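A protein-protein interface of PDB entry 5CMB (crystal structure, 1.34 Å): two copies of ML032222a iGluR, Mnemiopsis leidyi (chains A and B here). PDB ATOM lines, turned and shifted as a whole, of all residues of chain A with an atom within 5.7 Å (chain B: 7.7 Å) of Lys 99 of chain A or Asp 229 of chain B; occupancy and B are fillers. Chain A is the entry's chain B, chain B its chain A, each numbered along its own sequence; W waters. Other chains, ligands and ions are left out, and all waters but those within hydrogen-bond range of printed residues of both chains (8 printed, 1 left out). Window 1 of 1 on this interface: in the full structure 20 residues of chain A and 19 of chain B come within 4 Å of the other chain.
Of the printed residues of chain B, Lys 99 of chain A touches Ser 226 (3.7 Å), Asp 229 (3.8 Å), Ser 230 (3.0 Å) and Leu 233 (3.6 Å).
Printed residues of chain A within 4 Å of Asp 229 of chain B: Lys 99.
Of the printed residues of chain A, Leu 233 of chain B touches Asn 95 (3.6 Å), Ser 96 (3.99 Å) and Lys 99 (3.6 Å).
Of the printed residues of chain A, Lys 234 of chain B touches Ser 96.
Printed residues of chain B within 4 Å of Ser 96 of chain A: Leu 233 (3.99 Å), Lys 234 (3.6 Å) and Glu 237 (2.9 Å).
Of the printed residues of chain B, Asn 95 of chain A touches Leu 233 and Glu 237.
Printed residues of chain A within 4 Å of Glu 237 of chain B: Asn 95 (3.2 Å) and Ser 96 (2.9 Å).
Asp 103 of chain A touches none of the printed residues of chain B.
Of the 23 printed residues of chain B, 6 touch a printed residue of chain A.
Hydrophobic or aromatic side chains of chain B that line the printed part of chain A: Leu 233.
Of the 12 printed residues of chain A, 3 touch a printed residue of chain B.
Among the printed residues, 9 pairs touch across the chains.
Among the printed residues, no Asp or Glu carboxylate lies within 4 Å of a Lys or Arg side-chain nitrogen of the other chain.
Water W8 lies within hydrogen-bond range of the side-chain carboxylate (OD1) of Asp 103 of chain A (2.7 Å) and the side-chain hydroxyl (OG) of Ser 226 of chain B (2.7 Å).
Water W3 lies within hydrogen-bond range of OE2 of Glu 237 of chain B, N of Ala 97 of chain A and N of Ser 96 of chain A.
Water W2 lies within hydrogen-bond range of the side-chain hydroxyl (OG) of Ser 96 of chain A and the backbone carbonyl oxygen (O) of Ser 230 of chain B.
Water W7 lies within hydrogen-bond range of the backbone carbonyl oxygen of Lys 99 of chain A (2.8 Å), the side-chain amino group of Lys 220 of chain A (2.9 Å) and the side-chain hydroxyl of Ser 230 of chain B (3.3 Å).
Water W6 lies within hydrogen-bond range of the side-chain amino group (NZ) of Lys 225 of chain A (2.8 Å), the backbone carbonyl oxygen (O) of Tyr 104 of chain A (3.4 Å), the side-chain amino group (NZ) of Lys 225 of chain B (3.4 Å) and the side-chain carboxylate (OD2) of Asp 229 of chain B (3.4 Å).
Water W1 bridges OE2 of Glu 237 of chain B and OG of Ser 96 of chain A.
Asn 95 of chain A touches Leu 233 of chain B.
Asn 95 of chain A touches Glu 237 of chain B.
N of Ser 96 of chain A touches CD2 of Leu 233 of chain B (3.99 Å).
Ser 96 of chain A touches Lys 234 of chain B.
Ser 226 of chain B touches Lys 99 of chain A.
Asp 229 of chain B touches Lys 99 of chain A.
CD2 of Leu 233 of chain B touches CB of Lys 99 of chain A, at 3.6 Å.
N of Ser 96 of chain A is in hydrogen-bond range of OE1 of Glu 237 of chain B.
The side-chain hydroxyl (OG) of Ser 230 of chain B is in hydrogen-bond range of the side-chain amino group (NZ) of Lys 99 of chain A (3.0 Å).
The side-chain amide oxygen of Asn 95 of chain A lies close to the backbone NH of Ala 97 of chain A (3.3 Å).
The backbone carbonyl oxygen of Ser 226 of chain B lies within hydrogen-bond range of the side-chain hydroxyl of Ser 230 of chain B (3.3 Å).
The side-chain hydroxyl (OH) of Tyr 104 of chain A lies within hydrogen-bond range of the backbone NH (N) of Asn 95 of chain A.
NZ of Lys 225 of chain B lies within salt-bridge range of OD2 of Asp 229 of chain B (2.7 Å).
OD1 of Asp 229 of chain B sits at hydrogen-bond distance from N of Phe 106 of chain B, at 2.8 Å.
The side-chain amide oxygen of Asn 95 of chain A lies within hydrogen-bond range of the backbone NH of Arg 98 of chain A.
2 positions are printed for both chains.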
ATOM      1  N   ASN A  95      22.048   8.598   7.953  1.00  0.00           N
ATOM      2  CA  ASN A  95      20.600   8.407   8.007  1.00  0.00           C
ATOM      3  C   ASN A  95      20.259   7.026   7.480  1.00  0.00           C
ATOM      4  O   ASN A  95      21.031   6.400   6.753  1.00  0.00           O
ATOM      5  CB  ASN A  95      19.776   9.554   7.377  1.00  0.00           C
ATOM      6  CG  ASN A  95      19.939   9.686   5.885  1.00  0.00           C
ATOM      7  OD1 ASN A  95      19.755   8.721   5.151  1.00  0.00           O
ATOM      8  ND2 ASN A  95      20.213  10.903   5.419  1.00  0.00           N
ATOM      9  N   SER A  96      19.106   6.516   7.908  1.00  0.00           N
ATOM     10  CA  SER A  96      18.733   5.159   7.556  1.00  0.00           C
ATOM     11  C   SER A  96      18.476   4.963   6.072  1.00  0.00           C
ATOM     12  O   SER A  96      18.741   3.892   5.542  1.00  0.00           O
ATOM     13  CB  SER A  96      17.510   4.724   8.338  1.00  0.00           C
ATOM     14  OG  SER A  96      17.809   4.661   9.725  1.00  0.00           O
ATOM     15  N   ALA A  97      17.954   5.982   5.408  1.00  0.00           N
ATOM     16  CA  ALA A  97      17.736   5.862   3.965  1.00  0.00           C
ATOM     17  C   ALA A  97      19.054   5.552   3.240  1.00  0.00           C
ATOM     18  O   ALA A  97      19.173   4.616   2.467  1.00  0.00           O
ATOM     19  CB  ALA A  97      17.086   7.130   3.403  1.00  0.00           C
ATOM     20  N   ARG A  98      20.090   6.319   3.556  1.00  0.00           N
ATOM     21  CA  ARG A  98      21.392   6.092   2.951  1.00  0.00           C
ATOM     22  C   ARG A  98      21.989   4.753   3.363  1.00  0.00           C
ATOM     23  O   ARG A  98      22.609   4.074   2.563  1.00  0.00           O
ATOM     24  CB  ARG A  98      22.344   7.222   3.345  1.00  0.00           C
ATOM     25  CG  ARG A  98      22.035   8.526   2.631  1.00  0.00           C
ATOM     26  CD  ARG A  98      22.769   9.693   3.235  1.00  0.00           C
ATOM     27  NE  ARG A  98      22.549  10.914   2.473  1.00  0.00           N
ATOM     28  CZ  ARG A  98      23.010  12.099   2.822  1.00  0.00           C
ATOM     29  NH1 ARG A  98      23.716  12.241   3.937  1.00  0.00           N
ATOM     30  NH2 ARG A  98      22.792  13.152   2.055  1.00  0.00           N
ATOM     31  N   LYS A  99      21.799   4.398   4.628  1.00  0.00           N
ATOM     32  CA  LYS A  99      22.347   3.167   5.174  1.00  0.00           C
ATOM     33  C   LYS A  99      21.799   1.945   4.442  1.00  0.00           C
ATOM     34  O   LYS A  99      22.447   0.922   4.396  1.00  0.00           O
ATOM     35  CB  LYS A  99      22.041   3.095   6.666  1.00  0.00           C
ATOM     36  CG  LYS A  99      22.665   1.921   7.405  1.00  0.00           C
ATOM     37  CD  LYS A  99      24.198   2.019   7.504  1.00  0.00           C
ATOM     38  CE  LYS A  99      24.773   0.913   8.335  1.00  0.00           C
ATOM     39  NZ  LYS A  99      24.518  -0.372   7.730  1.00  0.00           N
ATOM     40  N   SER A 100      20.607   2.045   3.861  1.00  0.00           N
ATOM     41  CA  SER A 100      20.080   0.909   3.097  1.00  0.00           C
ATOM     42  C   SER A 100      20.915   0.669   1.829  1.00  0.00           C
ATOM     43  O   SER A 100      21.011  -0.461   1.336  1.00  0.00           O
ATOM     44  CB  SER A 100      18.601   1.114   2.732  1.00  0.00           C
ATOM     45  OG  SER A 100      18.399   2.181   1.812  1.00  0.00           O
ATOM     46  N   ALA A 101      21.538   1.730   1.320  1.00  0.00           N
ATOM     47  CA  ALA A 101      22.260   1.673   0.039  1.00  0.00           C
ATOM     48  C   ALA A 101      23.790   1.684   0.132  1.00  0.00           C
ATOM     49  O   ALA A 101      24.448   1.139  -0.745  1.00  0.00           O
ATOM     50  CB  ALA A 101      21.809   2.815  -0.846  1.00  0.00           C
ATOM     51  N   ILE A 102      24.341   2.353   1.145  1.00  0.00           N
ATOM     52  CA  ILE A 102      25.794   2.508   1.318  1.00  0.00           C
ATOM     53  C   ILE A 102      26.178   2.216   2.749  1.00  0.00           C
ATOM     54  O   ILE A 102      25.306   2.118   3.622  1.00  0.00           O
ATOM     55  CB  ILE A 102      26.258   3.948   0.917  1.00  0.00           C
ATOM     56  CG1 ILE A 102      25.714   5.006   1.873  1.00  0.00           C
ATOM     57  CG2 ILE A 102      25.902   4.234  -0.567  1.00  0.00           C
ATOM     58  CD1 ILE A 102      26.603   6.243   1.919  1.00  0.00           C
ATOM     59  N   ASP A 103      27.477   2.109   2.985  1.00  0.00           N
ATOM     60  CA  ASP A 103      28.019   2.060   4.322  1.00  0.00           C
ATOM     61  C   ASP A 103      28.584   3.427   4.707  1.00  0.00           C
ATOM     62  O   ASP A 103      28.762   4.325   3.874  1.00  0.00           O
ATOM     63  CB  ASP A 103      29.125   1.006   4.442  1.00  0.00           C
ATOM     64  CG  ASP A 103      28.599  -0.424   4.483  1.00  0.00           C
ATOM     65  OD1 ASP A 103      27.384  -0.645   4.674  1.00  0.00           O
ATOM     66  OD2 ASP A 103      29.450  -1.331   4.371  1.00  0.00           O
ATOM     67  N   TYR A 104      28.870   3.562   5.992  1.00  0.00           N
ATOM     68  CA  TYR A 104      29.551   4.724   6.508  1.00  0.00           C
ATOM     69  C   TYR A 104      30.863   4.295   7.123  1.00  0.00           C
ATOM     70  O   TYR A 104      30.992   3.175   7.644  1.00  0.00           O
ATOM     71  CB  TYR A 104      28.716   5.423   7.563  1.00  0.00           C
ATOM     72  CG  TYR A 104      27.512   6.133   7.032  1.00  0.00           C
ATOM     73  CD1 TYR A 104      27.630   7.413   6.521  1.00  0.00           C
ATOM     74  CD2 TYR A 104      26.250   5.552   7.068  1.00  0.00           C
ATOM     75  CE1 TYR A 104      26.533   8.116   6.079  1.00  0.00           C
ATOM     76  CE2 TYR A 104      25.130   6.250   6.614  1.00  0.00           C
ATOM     77  CZ  TYR A 104      25.281   7.523   6.108  1.00  0.00           C
ATOM     78  OH  TYR A 104      24.164   8.204   5.708  1.00  0.00           O
ATOM     79  N   LYS A 220      29.043  -0.461  -0.176  1.00  0.00           N
ATOM     80  CA  LYS A 220      28.988  -1.774   0.441  1.00  0.00           C
ATOM     81  C   LYS A 220      30.055  -2.651  -0.207  1.00  0.00           C
ATOM     82  O   LYS A 220      30.307  -2.555  -1.412  1.00  0.00           O
ATOM     83  CB  LYS A 220      27.598  -2.395   0.298  1.00  0.00           C
ATOM     84  CG  LYS A 220      26.547  -1.661   1.124  1.00  0.00           C
ATOM     85  CD  LYS A 220      25.172  -2.304   0.993  1.00  0.00           C
ATOM     86  CE  LYS A 220      24.209  -1.632   1.946  1.00  0.00           C
ATOM     87  NZ  LYS A 220      22.989  -2.441   2.221  1.00  0.00           N
ATOM     88  N   LYS A 225      37.226  -0.140   3.740  1.00  0.00           N
ATOM     89  CA  LYS A 225      36.507   0.340   4.915  1.00  0.00           C
ATOM     90  C   LYS A 225      37.252   0.097   6.222  1.00  0.00           C
ATOM     91  O   LYS A 225      37.345   0.983   7.065  1.00  0.00           O
ATOM     92  CB  LYS A 225      35.106  -0.293   4.998  1.00  0.00           C
ATOM     93  CG  LYS A 225      34.365   0.040   6.295  1.00  0.00           C
ATOM     94  CD  LYS A 225      32.873  -0.282   6.228  1.00  0.00           C
ATOM     95  CE  LYS A 225      32.198  -0.314   7.611  1.00  0.00           C
ATOM     96  NZ  LYS A 225      32.428   0.888   8.438  1.00  0.00           N
ATOM     97  N   LEU B  45      16.467  -5.288  19.539  1.00  0.00           N
ATOM     98  CA  LEU B  45      17.157  -5.920  18.423  1.00  0.00           C
ATOM     99  C   LEU B  45      16.664  -7.354  18.224  1.00  0.00           C
ATOM    100  O   LEU B  45      16.430  -7.772  17.089  1.00  0.00           O
ATOM    101  CB  LEU B  45      18.670  -5.932  18.646  1.00  0.00           C
ATOM    102  CG  LEU B  45      19.404  -4.610  18.532  1.00  0.00           C
ATOM    103  CD1 LEU B  45      20.831  -4.742  19.045  1.00  0.00           C
ATOM    104  CD2 LEU B  45      19.401  -4.122  17.095  1.00  0.00           C
ATOM    105  N   LEU B  49      14.937  -8.455  14.759  1.00  0.00           N
ATOM    106  CA  LEU B  49      15.799  -9.261  13.906  1.00  0.00           C
ATOM    107  C   LEU B  49      15.547 -10.750  14.052  1.00  0.00           C
ATOM    108  O   LEU B  49      15.962 -11.541  13.203  1.00  0.00           O
ATOM    109  CB  LEU B  49      17.282  -8.924  14.169  1.00  0.00           C
ATOM    110  CG  LEU B  49      17.676  -7.539  13.633  1.00  0.00           C
ATOM    111  CD1 LEU B  49      18.990  -7.051  14.230  1.00  0.00           C
ATOM    112  CD2 LEU B  49      17.765  -7.576  12.106  1.00  0.00           C
ATOM    113  N   MET B  87      29.096 -11.247  20.008  1.00  0.00           N
ATOM    114  CA  MET B  87      29.028  -9.804  20.039  1.00  0.00           C
ATOM    115  C   MET B  87      29.174  -9.382  21.489  1.00  0.00           C
ATOM    116  O   MET B  87      28.723 -10.121  22.390  1.00  0.00           O
ATOM    117  CB  MET B  87      27.680  -9.324  19.485  1.00  0.00           C
ATOM    118  CG  MET B  87      27.525  -7.779  19.419  1.00  0.00           C
ATOM    119  SD  MET B  87      26.111  -7.187  18.453  1.00  0.00           S
ATOM    120  CE  MET B  87      24.760  -7.521  19.573  1.00  0.00           C
ATOM    121  N   TYR B 104      33.864  -2.653  15.716  1.00  0.00           N
ATOM    122  CA  TYR B 104      32.799  -2.040  16.481  1.00  0.00           C
ATOM    123  C   TYR B 104      31.555  -1.915  15.626  1.00  0.00           C
ATOM    124  O   TYR B 104      31.646  -1.803  14.399  1.00  0.00           O
ATOM    125  CB  TYR B 104      33.207  -0.658  16.955  1.00  0.00           C
ATOM    126  CG  TYR B 104      34.256  -0.639  18.032  1.00  0.00           C
ATOM    127  CD1 TYR B 104      33.889  -0.802  19.356  1.00  0.00           C
ATOM    128  CD2 TYR B 104      35.595  -0.415  17.740  1.00  0.00           C
ATOM    129  CE1 TYR B 104      34.829  -0.759  20.365  1.00  0.00           C
ATOM    130  CE2 TYR B 104      36.537  -0.372  18.731  1.00  0.00           C
ATOM    131  CZ  TYR B 104      36.150  -0.559  20.037  1.00  0.00           C
ATOM    132  OH  TYR B 104      37.101  -0.448  21.027  1.00  0.00           O
ATOM    133  N   SER B 105      30.402  -1.907  16.278  1.00  0.00           N
ATOM    134  CA  SER B 105      29.166  -1.553  15.618  1.00  0.00           C
ATOM    135  C   SER B 105      29.129  -0.052  15.407  1.00  0.00           C
ATOM    136  O   SER B 105      29.960   0.695  15.931  1.00  0.00           O
ATOM    137  CB  SER B 105      27.954  -1.949  16.470  1.00  0.00           C
ATOM    138  OG  SER B 105      27.840  -1.132  17.617  1.00  0.00           O
ATOM    139  N   PHE B 106      28.093   0.392  14.698  1.00  0.00           N
ATOM    140  CA  PHE B 106      27.727   1.792  14.693  1.00  0.00           C
ATOM    141  C   PHE B 106      27.583   2.254  16.136  1.00  0.00           C
ATOM    142  O   PHE B 106      27.062   1.525  16.966  1.00  0.00           O
ATOM    143  CB  PHE B 106      26.396   1.975  13.963  1.00  0.00           C
ATOM    144  CG  PHE B 106      26.082   3.403  13.641  1.00  0.00           C
ATOM    145  CD1 PHE B 106      26.647   4.004  12.539  1.00  0.00           C
ATOM    146  CD2 PHE B 106      25.268   4.149  14.468  1.00  0.00           C
ATOM    147  CE1 PHE B 106      26.377   5.332  12.237  1.00  0.00           C
ATOM    148  CE2 PHE B 106      25.004   5.487  14.181  1.00  0.00           C
ATOM    149  CZ  PHE B 106      25.567   6.068  13.061  1.00  0.00           C
ATOM    150  N   PRO B 107      28.094   3.440  16.482  1.00  0.00           N
ATOM    151  CA  PRO B 107      28.108   3.871  17.877  1.00  0.00           C
ATOM    152  C   PRO B 107      26.773   4.439  18.334  1.00  0.00           C
ATOM    153  O   PRO B 107      25.989   4.868  17.491  1.00  0.00           O
ATOM    154  CB  PRO B 107      29.210   4.931  17.896  1.00  0.00           C
ATOM    155  CG  PRO B 107      29.218   5.487  16.520  1.00  0.00           C
ATOM    156  CD  PRO B 107      28.849   4.354  15.605  1.00  0.00           C
ATOM    157  N   ALA B 215      29.906   1.701  21.740  1.00  0.00           N
ATOM    158  CA  ALA B 215      29.386   0.896  20.668  1.00  0.00           C
ATOM    159  C   ALA B 215      29.327  -0.549  21.174  1.00  0.00           C
ATOM    160  O   ALA B 215      29.697  -0.825  22.319  1.00  0.00           O
ATOM    161  CB  ALA B 215      30.297   1.015  19.449  1.00  0.00           C
ATOM    162  N   PHE B 216      28.848  -1.463  20.343  1.00  0.00           N
ATOM    163  CA  PHE B 216      28.979  -2.893  20.639  1.00  0.00           C
ATOM    164  C   PHE B 216      30.253  -3.413  19.953  1.00  0.00           C
ATOM    165  O   PHE B 216      30.747  -2.817  18.969  1.00  0.00           O
ATOM    166  CB  PHE B 216      27.756  -3.658  20.143  1.00  0.00           C
ATOM    167  CG  PHE B 216      26.496  -3.403  20.920  1.00  0.00           C
ATOM    168  CD1 PHE B 216      26.465  -2.669  22.104  1.00  0.00           C
ATOM    169  CD2 PHE B 216      25.311  -3.921  20.443  1.00  0.00           C
ATOM    170  CE1 PHE B 216      25.272  -2.501  22.799  1.00  0.00           C
ATOM    171  CE2 PHE B 216      24.131  -3.748  21.139  1.00  0.00           C
ATOM    172  CZ  PHE B 216      24.118  -3.016  22.306  1.00  0.00           C
ATOM    173  N   LEU B 218      32.227  -6.428  17.824  1.00  0.00           N
ATOM    174  CA  LEU B 218      31.954  -7.494  16.878  1.00  0.00           C
ATOM    175  C   LEU B 218      33.266  -8.119  16.422  1.00  0.00           C
ATOM    176  O   LEU B 218      34.276  -7.412  16.221  1.00  0.00           O
ATOM    177  CB  LEU B 218      31.199  -6.918  15.676  1.00  0.00           C
ATOM    178  CG  LEU B 218      29.737  -6.557  15.949  1.00  0.00           C
ATOM    179  CD1 LEU B 218      29.219  -5.513  14.962  1.00  0.00           C
ATOM    180  CD2 LEU B 218      28.911  -7.817  15.878  1.00  0.00           C
ATOM    181  N   TYR B 224      27.046 -10.567  11.062  1.00  0.00           N
ATOM    182  CA  TYR B 224      25.934  -9.848  11.669  1.00  0.00           C
ATOM    183  C   TYR B 224      26.146  -8.332  11.696  1.00  0.00           C
ATOM    184  O   TYR B 224      25.234  -7.598  12.065  1.00  0.00           O
ATOM    185  CB  TYR B 224      25.730 -10.350  13.079  1.00  0.00           C
ATOM    186  CG  TYR B 224      25.513 -11.842  13.173  1.00  0.00           C
ATOM    187  CD1 TYR B 224      24.686 -12.497  12.270  1.00  0.00           C
ATOM    188  CD2 TYR B 224      26.145 -12.586  14.153  1.00  0.00           C
ATOM    189  CE1 TYR B 224      24.481 -13.867  12.357  1.00  0.00           C
ATOM    190  CE2 TYR B 224      25.946 -13.961  14.250  1.00  0.00           C
ATOM    191  CZ  TYR B 224      25.115 -14.586  13.352  1.00  0.00           C
ATOM    192  OH  TYR B 224      24.924 -15.946  13.462  1.00  0.00           O
ATOM    193  N   LYS B 225      27.333  -7.873  11.326  1.00  0.00           N
ATOM    194  CA  LYS B 225      27.669  -6.458  11.526  1.00  0.00           C
ATOM    195  C   LYS B 225      26.752  -5.513  10.771  1.00  0.00           C
ATOM    196  O   LYS B 225      26.291  -4.518  11.319  1.00  0.00           O
ATOM    197  CB  LYS B 225      29.132  -6.154  11.177  1.00  0.00           C
ATOM    198  CG  LYS B 225      29.484  -4.663  11.245  1.00  0.00           C
ATOM    199  CD  LYS B 225      30.993  -4.391  11.252  1.00  0.00           C
ATOM    200  CE  LYS B 225      31.326  -2.942  10.883  1.00  0.00           C
ATOM    201  NZ  LYS B 225      30.736  -1.924  11.790  1.00  0.00           N
ATOM    202  N   SER B 226      26.501  -5.805   9.502  1.00  0.00           N
ATOM    203  CA  SER B 226      25.707  -4.896   8.685  1.00  0.00           C
ATOM    204  C   SER B 226      24.325  -4.693   9.288  1.00  0.00           C
ATOM    205  O   SER B 226      23.870  -3.556   9.399  1.00  0.00           O
ATOM    206  CB  SER B 226      25.583  -5.403   7.248  1.00  0.00           C
ATOM    207  OG  SER B 226      24.717  -4.559   6.494  1.00  0.00           O
ATOM    208  N   LEU B 227      23.659  -5.777   9.679  1.00  0.00           N
ATOM    209  CA  LEU B 227      22.324  -5.672  10.251  1.00  0.00           C
ATOM    210  C   LEU B 227      22.322  -4.989  11.608  1.00  0.00           C
ATOM    211  O   LEU B 227      21.457  -4.176  11.895  1.00  0.00           O
ATOM    212  CB  LEU B 227      21.658  -7.053  10.378  1.00  0.00           C
ATOM    213  CG  LEU B 227      21.045  -7.584   9.076  1.00  0.00           C
ATOM    214  CD1 LEU B 227      20.685  -9.056   9.230  1.00  0.00           C
ATOM    215  CD2 LEU B 227      19.827  -6.767   8.663  1.00  0.00           C
ATOM    216  N   ILE B 228      23.276  -5.326  12.469  1.00  0.00           N
ATOM    217  CA  ILE B 228      23.340  -4.670  13.763  1.00  0.00           C
ATOM    218  C   ILE B 228      23.558  -3.163  13.557  1.00  0.00           C
ATOM    219  O   ILE B 228      22.895  -2.325  14.187  1.00  0.00           O
ATOM    220  CB  ILE B 228      24.461  -5.279  14.637  1.00  0.00           C
ATOM    221  CG1 ILE B 228      24.127  -6.725  15.016  1.00  0.00           C
ATOM    222  CG2 ILE B 228      24.700  -4.440  15.876  1.00  0.00           C
ATOM    223  CD1 ILE B 228      22.886  -6.890  15.862  1.00  0.00           C
ATOM    224  N   ASP B 229      24.487  -2.819  12.675  1.00  0.00           N
ATOM    225  CA  ASP B 229      24.768  -1.407  12.395  1.00  0.00           C
ATOM    226  C   ASP B 229      23.523  -0.662  11.900  1.00  0.00           C
ATOM    227  O   ASP B 229      23.214   0.435  12.381  1.00  0.00           O
ATOM    228  CB  ASP B 229      25.859  -1.242  11.323  1.00  0.00           C
ATOM    229  CG  ASP B 229      27.268  -1.569  11.812  1.00  0.00           C
ATOM    230  OD1 ASP B 229      27.473  -1.769  13.035  1.00  0.00           O
ATOM    231  OD2 ASP B 229      28.174  -1.595  10.968  1.00  0.00           O
ATOM    232  N   SER B 230      22.813  -1.252  10.942  1.00  0.00           N
ATOM    233  CA  SER B 230      21.607  -0.620  10.401  1.00  0.00           C
ATOM    234  C   SER B 230      20.599  -0.368  11.495  1.00  0.00           C
ATOM    235  O   SER B 230      20.024   0.705  11.613  1.00  0.00           O
ATOM    236  CB  SER B 230      20.972  -1.507   9.342  1.00  0.00           C
ATOM    237  OG  SER B 230      21.717  -1.456   8.152  1.00  0.00           O
ATOM    238  N   HIS B 231      20.392  -1.375  12.333  1.00  0.00           N
ATOM    239  CA  HIS B 231      19.367  -1.278  13.345  1.00  0.00           C
ATOM    240  C   HIS B 231      19.761  -0.303  14.444  1.00  0.00           C
ATOM    241  O   HIS B 231      18.932   0.465  14.940  1.00  0.00           O
ATOM    242  CB  HIS B 231      18.967  -2.662  13.868  1.00  0.00           C
ATOM    243  CG  HIS B 231      18.092  -3.403  12.905  1.00  0.00           C
ATOM    244  ND1 HIS B 231      16.737  -3.548  13.098  1.00  0.00           N
ATOM    245  CD2 HIS B 231      18.364  -3.955  11.699  1.00  0.00           C
ATOM    246  CE1 HIS B 231      16.215  -4.197  12.071  1.00  0.00           C
ATOM    247  NE2 HIS B 231      17.176  -4.446  11.201  1.00  0.00           N
ATOM    248  N   LEU B 232      21.036  -0.269  14.813  1.00  0.00           N
ATOM    249  CA  LEU B 232      21.478   0.724  15.783  1.00  0.00           C
ATOM    250  C   LEU B 232      21.338   2.156  15.266  1.00  0.00           C
ATOM    251  O   LEU B 232      20.948   3.055  16.009  1.00  0.00           O
ATOM    252  CB  LEU B 232      22.914   0.446  16.227  1.00  0.00           C
ATOM    253  CG  LEU B 232      23.057  -0.766  17.159  1.00  0.00           C
ATOM    254  CD1 LEU B 232      24.530  -0.996  17.440  1.00  0.00           C
ATOM    255  CD2 LEU B 232      22.300  -0.634  18.453  1.00  0.00           C
ATOM    256  N   LEU B 233      21.652   2.365  13.993  1.00  0.00           N
ATOM    257  CA  LEU B 233      21.461   3.676  13.388  1.00  0.00           C
ATOM    258  C   LEU B 233      19.979   4.066  13.445  1.00  0.00           C
ATOM    259  O   LEU B 233      19.642   5.183  13.827  1.00  0.00           O
ATOM    260  CB  LEU B 233      21.996   3.696  11.958  1.00  0.00           C
ATOM    261  CG  LEU B 233      21.605   4.935  11.148  1.00  0.00           C
ATOM    262  CD1 LEU B 233      22.055   6.215  11.817  1.00  0.00           C
ATOM    263  CD2 LEU B 233      22.209   4.831   9.773  1.00  0.00           C
ATOM    264  N   LYS B 234      19.092   3.135  13.096  1.00  0.00           N
ATOM    265  CA  LYS B 234      17.667   3.410  13.145  1.00  0.00           C
ATOM    266  C   LYS B 234      17.236   3.758  14.569  1.00  0.00           C
ATOM    267  O   LYS B 234      16.449   4.670  14.772  1.00  0.00           O
ATOM    268  CB  LYS B 234      16.901   2.194  12.614  1.00  0.00           C
ATOM    269  CG  LYS B 234      15.395   2.335  12.592  1.00  0.00           C
ATOM    270  CD  LYS B 234      14.774   1.121  11.906  1.00  0.00           C
ATOM    271  CE  LYS B 234      13.253   1.153  11.945  1.00  0.00           C
ATOM    272  NZ  LYS B 234      12.642  -0.036  11.288  1.00  0.00           N
ATOM    273  N   PHE B 235      17.770   3.053  15.564  1.00  0.00           N
ATOM    274  CA  PHE B 235      17.440   3.377  16.957  1.00  0.00           C
ATOM    275  C   PHE B 235      17.801   4.833  17.249  1.00  0.00           C
ATOM    276  O   PHE B 235      17.057   5.562  17.915  1.00  0.00           O
ATOM    277  CB  PHE B 235      18.237   2.526  17.955  1.00  0.00           C
ATOM    278  CG  PHE B 235      17.790   1.077  18.107  1.00  0.00           C
ATOM    279  CD1 PHE B 235      16.711   0.549  17.419  1.00  0.00           C
ATOM    280  CD2 PHE B 235      18.493   0.252  18.953  1.00  0.00           C
ATOM    281  CE1 PHE B 235      16.337  -0.775  17.598  1.00  0.00           C
ATOM    282  CE2 PHE B 235      18.132  -1.068  19.138  1.00  0.00           C
ATOM    283  CZ  PHE B 235      17.066  -1.589  18.461  1.00  0.00           C
ATOM    284  N   GLU B 237      18.225   7.341  15.079  1.00  0.00           N
ATOM    285  CA  GLU B 237      17.416   8.231  14.245  1.00  0.00           C
ATOM    286  C   GLU B 237      15.979   8.381  14.749  1.00  0.00           C
ATOM    287  O   GLU B 237      15.412   9.466  14.644  1.00  0.00           O
ATOM    288  CB  GLU B 237      17.463   7.725  12.802  1.00  0.00           C
ATOM    289  CG  GLU B 237      16.682   8.559  11.807  1.00  0.00           C
ATOM    290  CD  GLU B 237      16.947   8.173  10.382  1.00  0.00           C
ATOM    291  OE1 GLU B 237      18.114   8.244   9.967  1.00  0.00           O
ATOM    292  OE2 GLU B 237      16.017   7.768   9.652  1.00  0.00           O
HETATM  293  O   HOH W   1      15.135   5.224  10.731  1.00  0.00           O
HETATM  294  O   HOH W   2      19.487   2.414   9.404  1.00  0.00           O
HETATM  295  O   HOH W   3      16.285   8.253   6.912  1.00  0.00           O
HETATM  296  O   HOH W   4      27.586  -1.375   8.354  1.00  0.00           O
HETATM  297  O   HOH W   5      32.386   0.275  11.660  1.00  0.00           O
HETATM  298  O   HOH W   6      30.203   1.081  10.188  1.00  0.00           O
HETATM  299  O   HOH W   7      22.170  -1.849   4.901  1.00  0.00           O
HETATM  300  O   HOH W   8      26.272  -3.110   4.782  1.00  0.00           O
